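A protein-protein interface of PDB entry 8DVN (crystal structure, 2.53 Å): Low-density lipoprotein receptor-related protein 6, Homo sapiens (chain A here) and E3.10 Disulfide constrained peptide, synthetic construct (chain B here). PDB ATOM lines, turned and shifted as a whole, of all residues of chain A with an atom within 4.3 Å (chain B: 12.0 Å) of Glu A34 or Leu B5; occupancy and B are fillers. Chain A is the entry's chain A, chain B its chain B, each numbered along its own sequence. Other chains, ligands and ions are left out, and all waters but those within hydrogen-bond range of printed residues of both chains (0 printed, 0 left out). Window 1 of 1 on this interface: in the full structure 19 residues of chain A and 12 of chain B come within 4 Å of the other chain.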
ATOM      1  N   ARG A  10      -2.220  19.267  22.248  1.00  0.00           N
ATOM      2  CA  ARG A  10      -3.162  18.844  21.220  1.00  0.00           C
ATOM      3  C   ARG A  10      -2.441  18.074  20.122  1.00  0.00           C
ATOM      4  O   ARG A  10      -1.863  17.009  20.373  1.00  0.00           O
ATOM      5  CB  ARG A  10      -3.899  20.050  20.636  1.00  0.00           C
ATOM      6  CG  ARG A  10      -4.675  20.833  21.664  1.00  0.00           C
ATOM      7  CD  ARG A  10      -5.936  20.089  22.049  1.00  0.00           C
ATOM      8  NE  ARG A  10      -6.655  20.752  23.130  1.00  0.00           N
ATOM      9  CZ  ARG A  10      -7.777  20.299  23.669  1.00  0.00           C
ATOM     10  NH1 ARG A  10      -8.343  19.179  23.251  1.00  0.00           N
ATOM     11  NH2 ARG A  10      -8.350  20.993  24.649  1.00  0.00           N
ATOM     12  N   VAL A  32      -0.120  14.864  12.484  1.00  0.00           N
ATOM     13  CA  VAL A  32      -0.180  14.561  13.910  1.00  0.00           C
ATOM     14  C   VAL A  32      -1.601  14.817  14.396  1.00  0.00           C
ATOM     15  O   VAL A  32      -2.164  15.890  14.151  1.00  0.00           O
ATOM     16  CB  VAL A  32       0.833  15.408  14.700  1.00  0.00           C
ATOM     17  CG1 VAL A  32       0.577  15.284  16.196  1.00  0.00           C
ATOM     18  CG2 VAL A  32       2.261  15.001  14.362  1.00  0.00           C
ATOM     19  N   LYS A  33      -2.185  13.835  15.084  1.00  0.00           N
ATOM     20  CA  LYS A  33      -3.536  13.975  15.611  1.00  0.00           C
ATOM     21  C   LYS A  33      -3.597  14.208  17.115  1.00  0.00           C
ATOM     22  O   LYS A  33      -4.496  14.915  17.576  1.00  0.00           O
ATOM     23  CB  LYS A  33      -4.377  12.746  15.250  1.00  0.00           C
ATOM     24  CG  LYS A  33      -4.788  12.722  13.778  1.00  0.00           C
ATOM     25  CD  LYS A  33      -6.276  12.433  13.608  1.00  0.00           C
ATOM     26  CE  LYS A  33      -6.885  13.222  12.446  1.00  0.00           C
ATOM     27  NZ  LYS A  33      -5.937  13.452  11.320  1.00  0.00           N
ATOM     28  N   GLU A  34      -2.685  13.636  17.902  1.00  0.00           N
ATOM     29  CA  GLU A  34      -2.611  13.984  19.321  1.00  0.00           C
ATOM     30  C   GLU A  34      -1.202  13.650  19.812  1.00  0.00           C
ATOM     31  O   GLU A  34      -0.926  12.499  20.160  1.00  0.00           O
ATOM     32  CB  GLU A  34      -3.677  13.253  20.119  1.00  0.00           C
ATOM     33  CG  GLU A  34      -3.717  13.609  21.591  1.00  0.00           C
ATOM     34  CD  GLU A  34      -4.755  12.803  22.355  1.00  0.00           C
ATOM     35  OE1 GLU A  34      -5.128  11.702  21.881  1.00  0.00           O
ATOM     36  OE2 GLU A  34      -5.197  13.276  23.429  1.00  0.00           O
ATOM     37  N   ALA A  35      -0.339  14.659  19.869  1.00  0.00           N
ATOM     38  CA  ALA A  35       1.048  14.452  20.268  1.00  0.00           C
ATOM     39  C   ALA A  35       1.127  14.358  21.784  1.00  0.00           C
ATOM     40  O   ALA A  35       0.673  15.270  22.484  1.00  0.00           O
ATOM     41  CB  ALA A  35       1.926  15.590  19.753  1.00  0.00           C
ATOM     42  N   SER A  36       1.692  13.258  22.300  1.00  0.00           N
ATOM     43  CA  SER A  36       1.757  13.062  23.747  1.00  0.00           C
ATOM     44  C   SER A  36       3.184  13.027  24.284  1.00  0.00           C
ATOM     45  O   SER A  36       3.620  14.003  24.896  1.00  0.00           O
ATOM     46  CB  SER A  36       1.005  11.771  24.097  1.00  0.00           C
ATOM     47  OG  SER A  36       1.568  11.117  25.225  1.00  0.00           O
ATOM     48  N   THR A  50       5.071   9.971  20.503  1.00  0.00           N
ATOM     49  CA  THR A  50       3.938   9.061  20.425  1.00  0.00           C
ATOM     50  C   THR A  50       2.659   9.849  20.171  1.00  0.00           C
ATOM     51  O   THR A  50       2.560  11.040  20.473  1.00  0.00           O
ATOM     52  CB  THR A  50       3.784   8.234  21.708  1.00  0.00           C
ATOM     53  OG1 THR A  50       3.173   9.035  22.726  1.00  0.00           O
ATOM     54  CG2 THR A  50       5.141   7.738  22.197  1.00  0.00           C
ATOM     55  N   ASP A  51       1.674   9.161  19.603  1.00  0.00           N
ATOM     56  CA  ASP A  51       0.400   9.762  19.210  1.00  0.00           C
ATOM     57  C   ASP A  51      -0.704   8.831  19.702  1.00  0.00           C
ATOM     58  O   ASP A  51      -0.947   7.781  19.100  1.00  0.00           O
ATOM     59  CB  ASP A  51       0.345   9.960  17.703  1.00  0.00           C
ATOM     60  CG  ASP A  51      -0.825  10.798  17.264  1.00  0.00           C
ATOM     61  OD1 ASP A  51      -1.923  10.633  17.837  1.00  0.00           O
ATOM     62  OD2 ASP A  51      -0.649  11.614  16.330  1.00  0.00           O
ATOM     63  N   ILE A  52      -1.376   9.228  20.790  1.00  0.00           N
ATOM     64  CA  ILE A  52      -2.371   8.375  21.430  1.00  0.00           C
ATOM     65  C   ILE A  52      -3.633   8.223  20.591  1.00  0.00           C
ATOM     66  O   ILE A  52      -4.384   7.259  20.781  1.00  0.00           O
ATOM     67  CB  ILE A  52      -2.728   8.927  22.821  1.00  0.00           C
ATOM     68  CG1 ILE A  52      -1.456   9.291  23.584  1.00  0.00           C
ATOM     69  CG2 ILE A  52      -3.513   7.897  23.615  1.00  0.00           C
ATOM     70  CD1 ILE A  52      -0.545   8.106  23.856  1.00  0.00           C
ATOM     71  N   SER A  53      -3.903   9.141  19.669  1.00  0.00           N
ATOM     72  CA  SER A  53      -5.111   8.994  18.870  1.00  0.00           C
ATOM     73  C   SER A  53      -4.892   8.080  17.673  1.00  0.00           C
ATOM     74  O   SER A  53      -5.831   7.408  17.234  1.00  0.00           O
ATOM     75  CB  SER A  53      -5.620  10.367  18.424  1.00  0.00           C
ATOM     76  OG  SER A  53      -6.035  11.134  19.547  1.00  0.00           O
ATOM     77  N   TRP A 221      -1.811  22.094  34.607  1.00  0.00           N
ATOM     78  CA  TRP A 221      -3.017  22.160  33.789  1.00  0.00           C
ATOM     79  C   TRP A 221      -4.012  23.185  34.313  1.00  0.00           C
ATOM     80  O   TRP A 221      -4.808  23.725  33.534  1.00  0.00           O
ATOM     81  CB  TRP A 221      -3.676  20.794  33.726  1.00  0.00           C
ATOM     82  CG  TRP A 221      -2.988  19.869  32.820  1.00  0.00           C
ATOM     83  CD1 TRP A 221      -1.748  20.016  32.282  1.00  0.00           C
ATOM     84  CD2 TRP A 221      -3.506  18.642  32.318  1.00  0.00           C
ATOM     85  NE1 TRP A 221      -1.456  18.948  31.474  1.00  0.00           N
ATOM     86  CE2 TRP A 221      -2.522  18.086  31.482  1.00  0.00           C
ATOM     87  CE3 TRP A 221      -4.707  17.957  32.498  1.00  0.00           C
ATOM     88  CZ2 TRP A 221      -2.702  16.872  30.833  1.00  0.00           C
ATOM     89  CZ3 TRP A 221      -4.881  16.754  31.853  1.00  0.00           C
ATOM     90  CH2 TRP A 221      -3.891  16.224  31.030  1.00  0.00           C
ATOM     91  N   TYR A 246      -3.474  21.833  28.778  1.00  0.00           N
ATOM     92  CA  TYR A 246      -3.337  20.427  28.386  1.00  0.00           C
ATOM     93  C   TYR A 246      -2.046  20.190  27.610  1.00  0.00           C
ATOM     94  O   TYR A 246      -2.031  19.565  26.546  1.00  0.00           O
ATOM     95  CB  TYR A 246      -4.558  19.952  27.593  1.00  0.00           C
ATOM     96  CG  TYR A 246      -5.850  20.118  28.356  1.00  0.00           C
ATOM     97  CD1 TYR A 246      -6.049  19.482  29.582  1.00  0.00           C
ATOM     98  CD2 TYR A 246      -6.861  20.940  27.872  1.00  0.00           C
ATOM     99  CE1 TYR A 246      -7.230  19.652  30.292  1.00  0.00           C
ATOM    100  CE2 TYR A 246      -8.043  21.116  28.575  1.00  0.00           C
ATOM    101  CZ  TYR A 246      -8.222  20.472  29.779  1.00  0.00           C
ATOM    102  OH  TYR A 246      -9.400  20.653  30.463  1.00  0.00           O
ATOM    103  N   GLY B   1      -7.829  14.911  17.692  1.00  0.00           N
ATOM    104  CA  GLY B   1      -7.989  13.715  18.496  1.00  0.00           C
ATOM    105  C   GLY B   1      -7.836  13.999  19.973  1.00  0.00           C
ATOM    106  O   GLY B   1      -7.055  14.865  20.367  1.00  0.00           O
ATOM    107  N   CYS B   2      -8.584  13.270  20.798  1.00  0.00           N
ATOM    108  CA  CYS B   2      -8.539  13.492  22.238  1.00  0.00           C
ATOM    109  C   CYS B   2      -8.475  12.182  23.004  1.00  0.00           C
ATOM    110  O   CYS B   2      -8.804  12.157  24.196  1.00  0.00           O
ATOM    111  CB  CYS B   2      -9.752  14.287  22.705  1.00  0.00           C
ATOM    112  SG  CYS B   2     -11.237  13.785  21.853  1.00  0.00           S
ATOM    113  N   ARG B   3      -8.059  11.097  22.350  1.00  0.00           N
ATOM    114  CA  ARG B   3      -8.051   9.793  22.997  1.00  0.00           C
ATOM    115  C   ARG B   3      -7.186   9.803  24.250  1.00  0.00           C
ATOM    116  O   ARG B   3      -7.592   9.288  25.298  1.00  0.00           O
ATOM    117  CB  ARG B   3      -7.557   8.744  22.007  1.00  0.00           C
ATOM    118  CG  ARG B   3      -8.230   7.411  22.115  1.00  0.00           C
ATOM    119  CD  ARG B   3      -7.797   6.523  20.978  1.00  0.00           C
ATOM    120  NE  ARG B   3      -7.873   5.116  21.357  1.00  0.00           N
ATOM    121  CZ  ARG B   3      -6.985   4.498  22.122  1.00  0.00           C
ATOM    122  NH1 ARG B   3      -5.923   5.130  22.597  1.00  0.00           N
ATOM    123  NH2 ARG B   3      -7.163   3.215  22.416  1.00  0.00           N
ATOM    124  N   GLY B   4      -5.994  10.393  24.165  1.00  0.00           N
ATOM    125  CA  GLY B   4      -5.129  10.448  25.333  1.00  0.00           C
ATOM    126  C   GLY B   4      -5.693  11.329  26.429  1.00  0.00           C
ATOM    127  O   GLY B   4      -5.758  10.927  27.595  1.00  0.00           O
ATOM    128  N   LEU B   5      -6.123  12.543  26.063  1.00  0.00           N
ATOM    129  CA  LEU B   5      -6.641  13.484  27.052  1.00  0.00           C
ATOM    130  C   LEU B   5      -7.928  12.969  27.687  1.00  0.00           C
ATOM    131  O   LEU B   5      -8.146  13.147  28.893  1.00  0.00           O
ATOM    132  CB  LEU B   5      -6.872  14.852  26.409  1.00  0.00           C
ATOM    133  CG  LEU B   5      -7.425  15.955  27.320  1.00  0.00           C
ATOM    134  CD1 LEU B   5      -6.658  16.020  28.633  1.00  0.00           C
ATOM    135  CD2 LEU B   5      -7.430  17.308  26.627  1.00  0.00           C
ATOM    136  N   LYS B   6      -8.797  12.337  26.889  1.00  0.00           N
ATOM    137  CA  LYS B   6     -10.013  11.751  27.442  1.00  0.00           C
ATOM    138  C   LYS B   6      -9.684  10.700  28.490  1.00  0.00           C
ATOM    139  O   LYS B   6     -10.286  10.683  29.567  1.00  0.00           O
ATOM    140  CB  LYS B   6     -10.859  11.145  26.322  1.00  0.00           C
ATOM    141  CG  LYS B   6     -12.043  10.320  26.784  1.00  0.00           C
ATOM    142  CD  LYS B   6     -12.709   9.655  25.581  1.00  0.00           C
ATOM    143  CE  LYS B   6     -14.022   8.972  25.941  1.00  0.00           C
ATOM    144  NZ  LYS B   6     -14.365   9.148  27.376  1.00  0.00           N
ATOM    145  N   ARG B   7      -8.707   9.838  28.205  1.00  0.00           N
ATOM    146  CA  ARG B   7      -8.341   8.794  29.155  1.00  0.00           C
ATOM    147  C   ARG B   7      -7.811   9.395  30.450  1.00  0.00           C
ATOM    148  O   ARG B   7      -8.105   8.898  31.544  1.00  0.00           O
ATOM    149  CB  ARG B   7      -7.315   7.859  28.517  1.00  0.00           C
ATOM    150  CG  ARG B   7      -7.073   6.565  29.268  1.00  0.00           C
ATOM    151  CD  ARG B   7      -5.584   6.357  29.518  1.00  0.00           C
ATOM    152  NE  ARG B   7      -5.351   5.830  30.854  1.00  0.00           N
ATOM    153  CZ  ARG B   7      -4.274   6.083  31.583  1.00  0.00           C
ATOM    154  NH1 ARG B   7      -3.288   6.834  31.122  1.00  0.00           N
ATOM    155  NH2 ARG B   7      -4.190   5.579  32.814  1.00  0.00           N
ATOM    156  N   LEU B   8      -7.026  10.471  30.342  1.00  0.00           N
ATOM    157  CA  LEU B   8      -6.528  11.153  31.531  1.00  0.00           C
ATOM    158  C   LEU B   8      -7.646  11.868  32.274  1.00  0.00           C
ATOM    159  O   LEU B   8      -7.638  11.920  33.510  1.00  0.00           O
ATOM    160  CB  LEU B   8      -5.436  12.153  31.157  1.00  0.00           C
ATOM    161  CG  LEU B   8      -4.112  11.591  30.660  1.00  0.00           C
ATOM    162  CD1 LEU B   8      -3.322  12.709  29.999  1.00  0.00           C
ATOM    163  CD2 LEU B   8      -3.348  10.977  31.815  1.00  0.00           C
ATOM    164  N   TYR B   9      -8.601  12.454  31.541  1.00  0.00           N
ATOM    165  CA  TYR B   9      -9.725  13.124  32.192  1.00  0.00           C
ATOM    166  C   TYR B   9     -10.531  12.143  33.038  1.00  0.00           C
ATOM    167  O   TYR B   9     -10.782  12.393  34.220  1.00  0.00           O
ATOM    168  CB  TYR B   9     -10.619  13.805  31.154  1.00  0.00           C
ATOM    169  CG  TYR B   9     -11.944  14.284  31.711  1.00  0.00           C
ATOM    170  CD1 TYR B   9     -11.992  15.180  32.772  1.00  0.00           C
ATOM    171  CD2 TYR B   9     -13.147  13.825  31.191  1.00  0.00           C
ATOM    172  CE1 TYR B   9     -13.199  15.617  33.292  1.00  0.00           C
ATOM    173  CE2 TYR B   9     -14.356  14.253  31.700  1.00  0.00           C
ATOM    174  CZ  TYR B   9     -14.381  15.150  32.752  1.00  0.00           C
ATOM    175  OH  TYR B   9     -15.590  15.581  33.264  1.00  0.00           O
ATOM    176  N   GLU B  10     -10.914  10.999  32.461  1.00  0.00           N
ATOM    177  CA  GLU B  10     -11.684  10.023  33.226  1.00  0.00           C
ATOM    178  C   GLU B  10     -10.879   9.368  34.337  1.00  0.00           C
ATOM    179  O   GLU B  10     -11.471   8.718  35.201  1.00  0.00           O
ATOM    180  CB  GLU B  10     -12.246   8.945  32.302  1.00  0.00           C
ATOM    181  CG  GLU B  10     -12.569   9.463  30.927  1.00  0.00           C
ATOM    182  CD  GLU B  10     -13.773   8.802  30.311  1.00  0.00           C
ATOM    183  OE1 GLU B  10     -13.787   7.553  30.233  1.00  0.00           O
ATOM    184  OE2 GLU B  10     -14.691   9.530  29.880  1.00  0.00           O
ATOM    185  N   ALA B  11      -9.556   9.512  34.339  1.00  0.00           N
ATOM    186  CA  ALA B  11      -8.744   8.936  35.399  1.00  0.00           C
ATOM    187  C   ALA B  11      -8.575   9.863  36.594  1.00  0.00           C
ATOM    188  O   ALA B  11      -8.126   9.408  37.653  1.00  0.00           O
ATOM    189  CB  ALA B  11      -7.367   8.549  34.854  1.00  0.00           C
ATOM    190  N   PHE B  12      -8.913  11.146  36.453  1.00  0.00           N
ATOM    191  CA  PHE B  12      -8.756  12.110  37.536  1.00  0.00           C
ATOM    192  C   PHE B  12      -9.979  13.009  37.717  1.00  0.00           C
ATOM    193  O   PHE B  12      -9.937  13.929  38.543  1.00  0.00           O
ATOM    194  CB  PHE B  12      -7.495  12.956  37.304  1.00  0.00           C
ATOM    195  CG  PHE B  12      -6.224  12.153  37.317  1.00  0.00           C
ATOM    196  CD1 PHE B  12      -5.536  11.935  38.502  1.00  0.00           C
ATOM    197  CD2 PHE B  12      -5.730  11.587  36.144  1.00  0.00           C
ATOM    198  CE1 PHE B  12      -4.370  11.178  38.518  1.00  0.00           C
ATOM    199  CE2 PHE B  12      -4.571  10.832  36.151  1.00  0.00           C
ATOM    200  CZ  PHE B  12      -3.888  10.629  37.341  1.00  0.00           C
ATOM    201  N   CYS B  13     -11.073  12.751  36.990  1.00  0.00           N
ATOM    202  CA  CYS B  13     -12.245  13.621  37.052  1.00  0.00           C
ATOM    203  C   CYS B  13     -12.942  13.544  38.404  1.00  0.00           C
ATOM    204  O   CYS B  13     -13.483  14.549  38.878  1.00  0.00           O
ATOM    205  CB  CYS B  13     -13.227  13.267  35.935  1.00  0.00           C
ATOM    206  SG  CYS B  13     -14.181  11.757  36.221  1.00  0.00           S
ATOM    207  N   LYS B  14     -12.932  12.374  39.044  1.00  0.00           N
ATOM    208  CA  LYS B  14     -13.581  12.224  40.339  1.00  0.00           C
ATOM    209  C   LYS B  14     -12.883  13.019  41.435  1.00  0.00           C
ATOM    210  O   LYS B  14     -13.415  13.118  42.546  1.00  0.00           O
ATOM    211  CB  LYS B  14     -13.652  10.741  40.708  1.00  0.00           C
ATOM    212  CG  LYS B  14     -14.419   9.910  39.683  1.00  0.00           C
ATOM    213  CD  LYS B  14     -14.455   8.432  40.037  1.00  0.00           C
ATOM    214  CE  LYS B  14     -15.284   7.655  39.018  1.00  0.00           C
ATOM    215  NZ  LYS B  14     -15.386   6.205  39.341  1.00  0.00           N
ATOM    216  N   ASP B  16     -12.741  16.128  41.899  1.00  0.00           N
ATOM    217  CA  ASP B  16     -13.313  17.437  41.624  1.00  0.00           C
ATOM    218  C   ASP B  16     -14.438  17.713  42.608  1.00  0.00           C
ATOM    219  O   ASP B  16     -15.126  16.792  43.057  1.00  0.00           O
ATOM    220  CB  ASP B  16     -13.835  17.538  40.185  1.00  0.00           C
ATOM    221  CG  ASP B  16     -12.724  17.788  39.177  1.00  0.00           C
ATOM    222  OD1 ASP B  16     -11.614  18.190  39.593  1.00  0.00           O
ATOM    223  OD2 ASP B  16     -12.961  17.583  37.966  1.00  0.00           O
ATOM    224  N   CYS B  25     -19.383  11.329  36.934  1.00  0.00           N
ATOM    225  CA  CYS B  25     -18.557  12.423  36.441  1.00  0.00           C
ATOM    226  C   CYS B  25     -19.009  12.982  35.094  1.00  0.00           C
ATOM    227  O   CYS B  25     -19.493  12.244  34.256  1.00  0.00           O
ATOM    228  CB  CYS B  25     -17.054  12.195  36.669  1.00  0.00           C
ATOM    229  SG  CYS B  25     -15.935  12.062  35.271  1.00  0.00           S
ATOM    230  N   PRO B  26     -18.839  14.293  34.868  1.00  0.00           N
ATOM    231  CA  PRO B  26     -19.454  14.829  33.645  1.00  0.00           C
ATOM    232  C   PRO B  26     -18.781  14.352  32.364  1.00  0.00           C
ATOM    233  O   PRO B  26     -17.609  13.967  32.339  1.00  0.00           O
ATOM    234  CB  PRO B  26     -19.297  16.347  33.805  1.00  0.00           C
ATOM    235  CG  PRO B  26     -19.036  16.563  35.266  1.00  0.00           C
ATOM    236  CD  PRO B  26     -18.285  15.359  35.720  1.00  0.00           C
ATOM    237  N   MET B  27     -19.555  14.407  31.277  1.00  0.00           N
ATOM    238  CA  MET B  27     -19.062  14.001  29.966  1.00  0.00           C
ATOM    239  C   MET B  27     -17.909  14.893  29.521  1.00  0.00           C
ATOM    240  O   MET B  27     -17.813  16.066  29.897  1.00  0.00           O
ATOM    241  CB  MET B  27     -20.187  14.051  28.927  1.00  0.00           C
ATOM    242  CG  MET B  27     -20.160  12.921  27.891  1.00  0.00           C
ATOM    243  SD  MET B  27     -21.236  13.195  26.451  1.00  0.00           S
ATOM    244  CE  MET B  27     -20.378  14.525  25.606  1.00  0.00           C
ATOM    245  N   PHE B  28     -17.025  14.319  28.711  1.00  0.00           N
ATOM    246  CA  PHE B  28     -15.831  15.014  28.250  1.00  0.00           C
ATOM    247  C   PHE B  28     -16.204  15.985  27.136  1.00  0.00           C
ATOM    248  O   PHE B  28     -16.737  15.573  26.100  1.00  0.00           O
ATOM    249  CB  PHE B  28     -14.795  14.002  27.773  1.00  0.00           C
ATOM    250  CG  PHE B  28     -13.466  14.603  27.445  1.00  0.00           C
ATOM    251  CD1 PHE B  28     -12.849  15.469  28.326  1.00  0.00           C
ATOM    252  CD2 PHE B  28     -12.836  14.306  26.249  1.00  0.00           C
ATOM    253  CE1 PHE B  28     -11.621  16.028  28.025  1.00  0.00           C
ATOM    254  CE2 PHE B  28     -11.609  14.860  25.938  1.00  0.00           C
ATOM    255  CZ  PHE B  28     -10.999  15.722  26.826  1.00  0.00           C
ATOM    256  N   SER B  29     -15.923  17.272  27.352  1.00  0.00           N
ATOM    257  CA  SER B  29     -16.269  18.319  26.400  1.00  0.00           C
ATOM    258  C   SER B  29     -15.055  19.014  25.802  1.00  0.00           C
ATOM    259  O   SER B  29     -15.222  19.893  24.947  1.00  0.00           O
ATOM    260  CB  SER B  29     -17.173  19.370  27.065  1.00  0.00           C
ATOM    261  OG  SER B  29     -16.663  19.769  28.328  1.00  0.00           O
ATOM    262  N   GLU B  30     -13.843  18.643  26.215  1.00  0.00           N
ATOM    263  CA  GLU B  30     -12.635  19.377  25.863  1.00  0.00           C
ATOM    264  C   GLU B  30     -11.931  18.829  24.631  1.00  0.00           C
ATOM    265  O   GLU B  30     -10.786  19.209  24.374  1.00  0.00           O
ATOM    266  CB  GLU B  30     -11.664  19.397  27.044  1.00  0.00           C
ATOM    267  CG  GLU B  30     -12.147  20.223  28.218  1.00  0.00           C
ATOM    268  CD  GLU B  30     -11.863  21.703  28.045  1.00  0.00           C
ATOM    269  OE1 GLU B  30     -11.362  22.099  26.970  1.00  0.00           O
ATOM    270  OE2 GLU B  30     -12.146  22.471  28.988  1.00  0.00           O
ATOM    271  N   CYS B  31     -12.568  17.939  23.880  1.00  0.00           N
ATOM    272  CA  CYS B  31     -12.033  17.580  22.576  1.00  0.00           C
ATOM    273  C   CYS B  31     -12.153  18.775  21.640  1.00  0.00           C
ATOM    274  O   CYS B  31     -13.207  19.414  21.564  1.00  0.00           O
ATOM    275  CB  CYS B  31     -12.771  16.377  22.000  1.00  0.00           C
ATOM    276  SG  CYS B  31     -11.799  15.430  20.808  1.00  0.00           S
ATOM    277  N   GLY B  32     -11.068  19.082  20.935  1.00  0.00           N
ATOM    278  CA  GLY B  32     -11.041  20.228  20.046  1.00  0.00           C
ATOM    279  C   GLY B  32     -10.166  21.356  20.560  1.00  0.00           C
ATOM    280  O   GLY B  32      -9.068  21.581  20.052  1.00  0.00           O
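NH2 of Arg A10 is in salt-bridge range of OE1 of Glu B30 (3.96 Å). The backbone NH (N) of Gly B1 sits at hydrogen-bond distance from the backbone carbonyl oxygen (O) of Lys A33 (3.3 Å). The side-chain carboxylate (OE1) of Glu A34 is in hydrogen-bond range of the backbone NH (N) of Arg B3, at 3.0 Å. The backbone NH (N) of Gly B4 is in hydrogen-bond range of the side-chain carboxylate (OE1) of Glu A34, at 2.8 Å. The side-chain carboxylate (OE2) of Glu A34 sits at hydrogen-bond distance from the backbone NH (N) of Leu B5 (2.9 Å). The backbone carbonyl oxygen (O) of Ile A52 sits at hydrogen-bond distance from the guanidinium group (NH1) of Arg B3, at 3.2 Å. N of Arg B3 is in hydrogen-bond range of OG of Ser A53.
N of Lys A33 sits at hydrogen-bond distance from OD2 of Asp A51 (3.0 Å). The backbone NH (N) of Glu A34 sits at hydrogen-bond distance from the side-chain carboxylate (OD1) of Asp A51, 3.1 Å away. The backbone carbonyl oxygen (O) of Glu A34 is in hydrogen-bond range of the backbone NH (N) of Ile A52 (3.4 Å). The side-chain carboxylate of Glu A34 is in hydrogen-bond range of the side-chain hydroxyl of Ser A53 (2.6 Å). SG of Cys B2 is disulfide-bonded to SG of Cys B31, at 2.0 Å. The side-chain sulfur (SG) of Cys B13 is disulfide-bonded to the side-chain sulfur (SG) of Cys B25 (2.0 Å).
Leu B5 touches Arg A10. Gly B32 touches Arg A10 (N to NH1, 3.6 Å). Gly B1 touches Glu A34. Gly B4 touches Ile A52. Ser A53 touches Gly B1. Ser A53 touches Cys B2. CH2 of Trp A221 touches CD1 of Leu B5, at 3.7 Å. Trp A221 touches Leu B8 (CH2 to CD1, 3.7 Å). CD1 of Tyr A246 touches CD1 of Leu B5, 3.6 Å away. Tyr A246 touches Glu B30 (OH to CG, 3.6 Å).
Of the printed residues of chain B, Arg A10 touches Leu B5 (3.97 Å), Glu B30 (2.7 Å) and Gly B32 (3.6 Å). No residue of chain B comes within 4 Å of Val A32. Of the printed residues of chain B, Glu A34 touches Gly B1, Cys B2, Arg B3, Gly B4 and Leu B5. No residue of chain B comes within 4 Å of Asp A51. Ser A53 touches three residues of chain B. Printed residues of chain B within 4 Å of Trp A221: Leu B5 (3.7 Å) and Leu B8 (3.7 Å). Tyr A246 touches two residues of chain B. Of the printed residues of chain A, Gly B4 touches Glu A34 and Ile A52. Of chain A, only Arg A10, Glu A34, Trp A221 and Tyr A246 come within 4 Å of Leu B5. Of the printed residues of chain A, Leu B8 touches Trp A221. Pro B26 touches none of the printed residues of chain A. Cys B31 touches none of the printed residues of chain A. The nearest residue of chain B that does not touch Glu A34 is Lys B6 (5.1 Å).
Of the 23 printed residues of chain B, 8 touch a printed residue of chain A. Hydrophobic or aromatic side chains of chain B within 4 Å of the printed part of chain A: Leu B5 and Leu B8. Printed residues of chain A that touch a printed residue of chain B: Arg A10, Lys A33, Glu A34, Ile A52, Ser A53, Trp A221 and Tyr A246.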
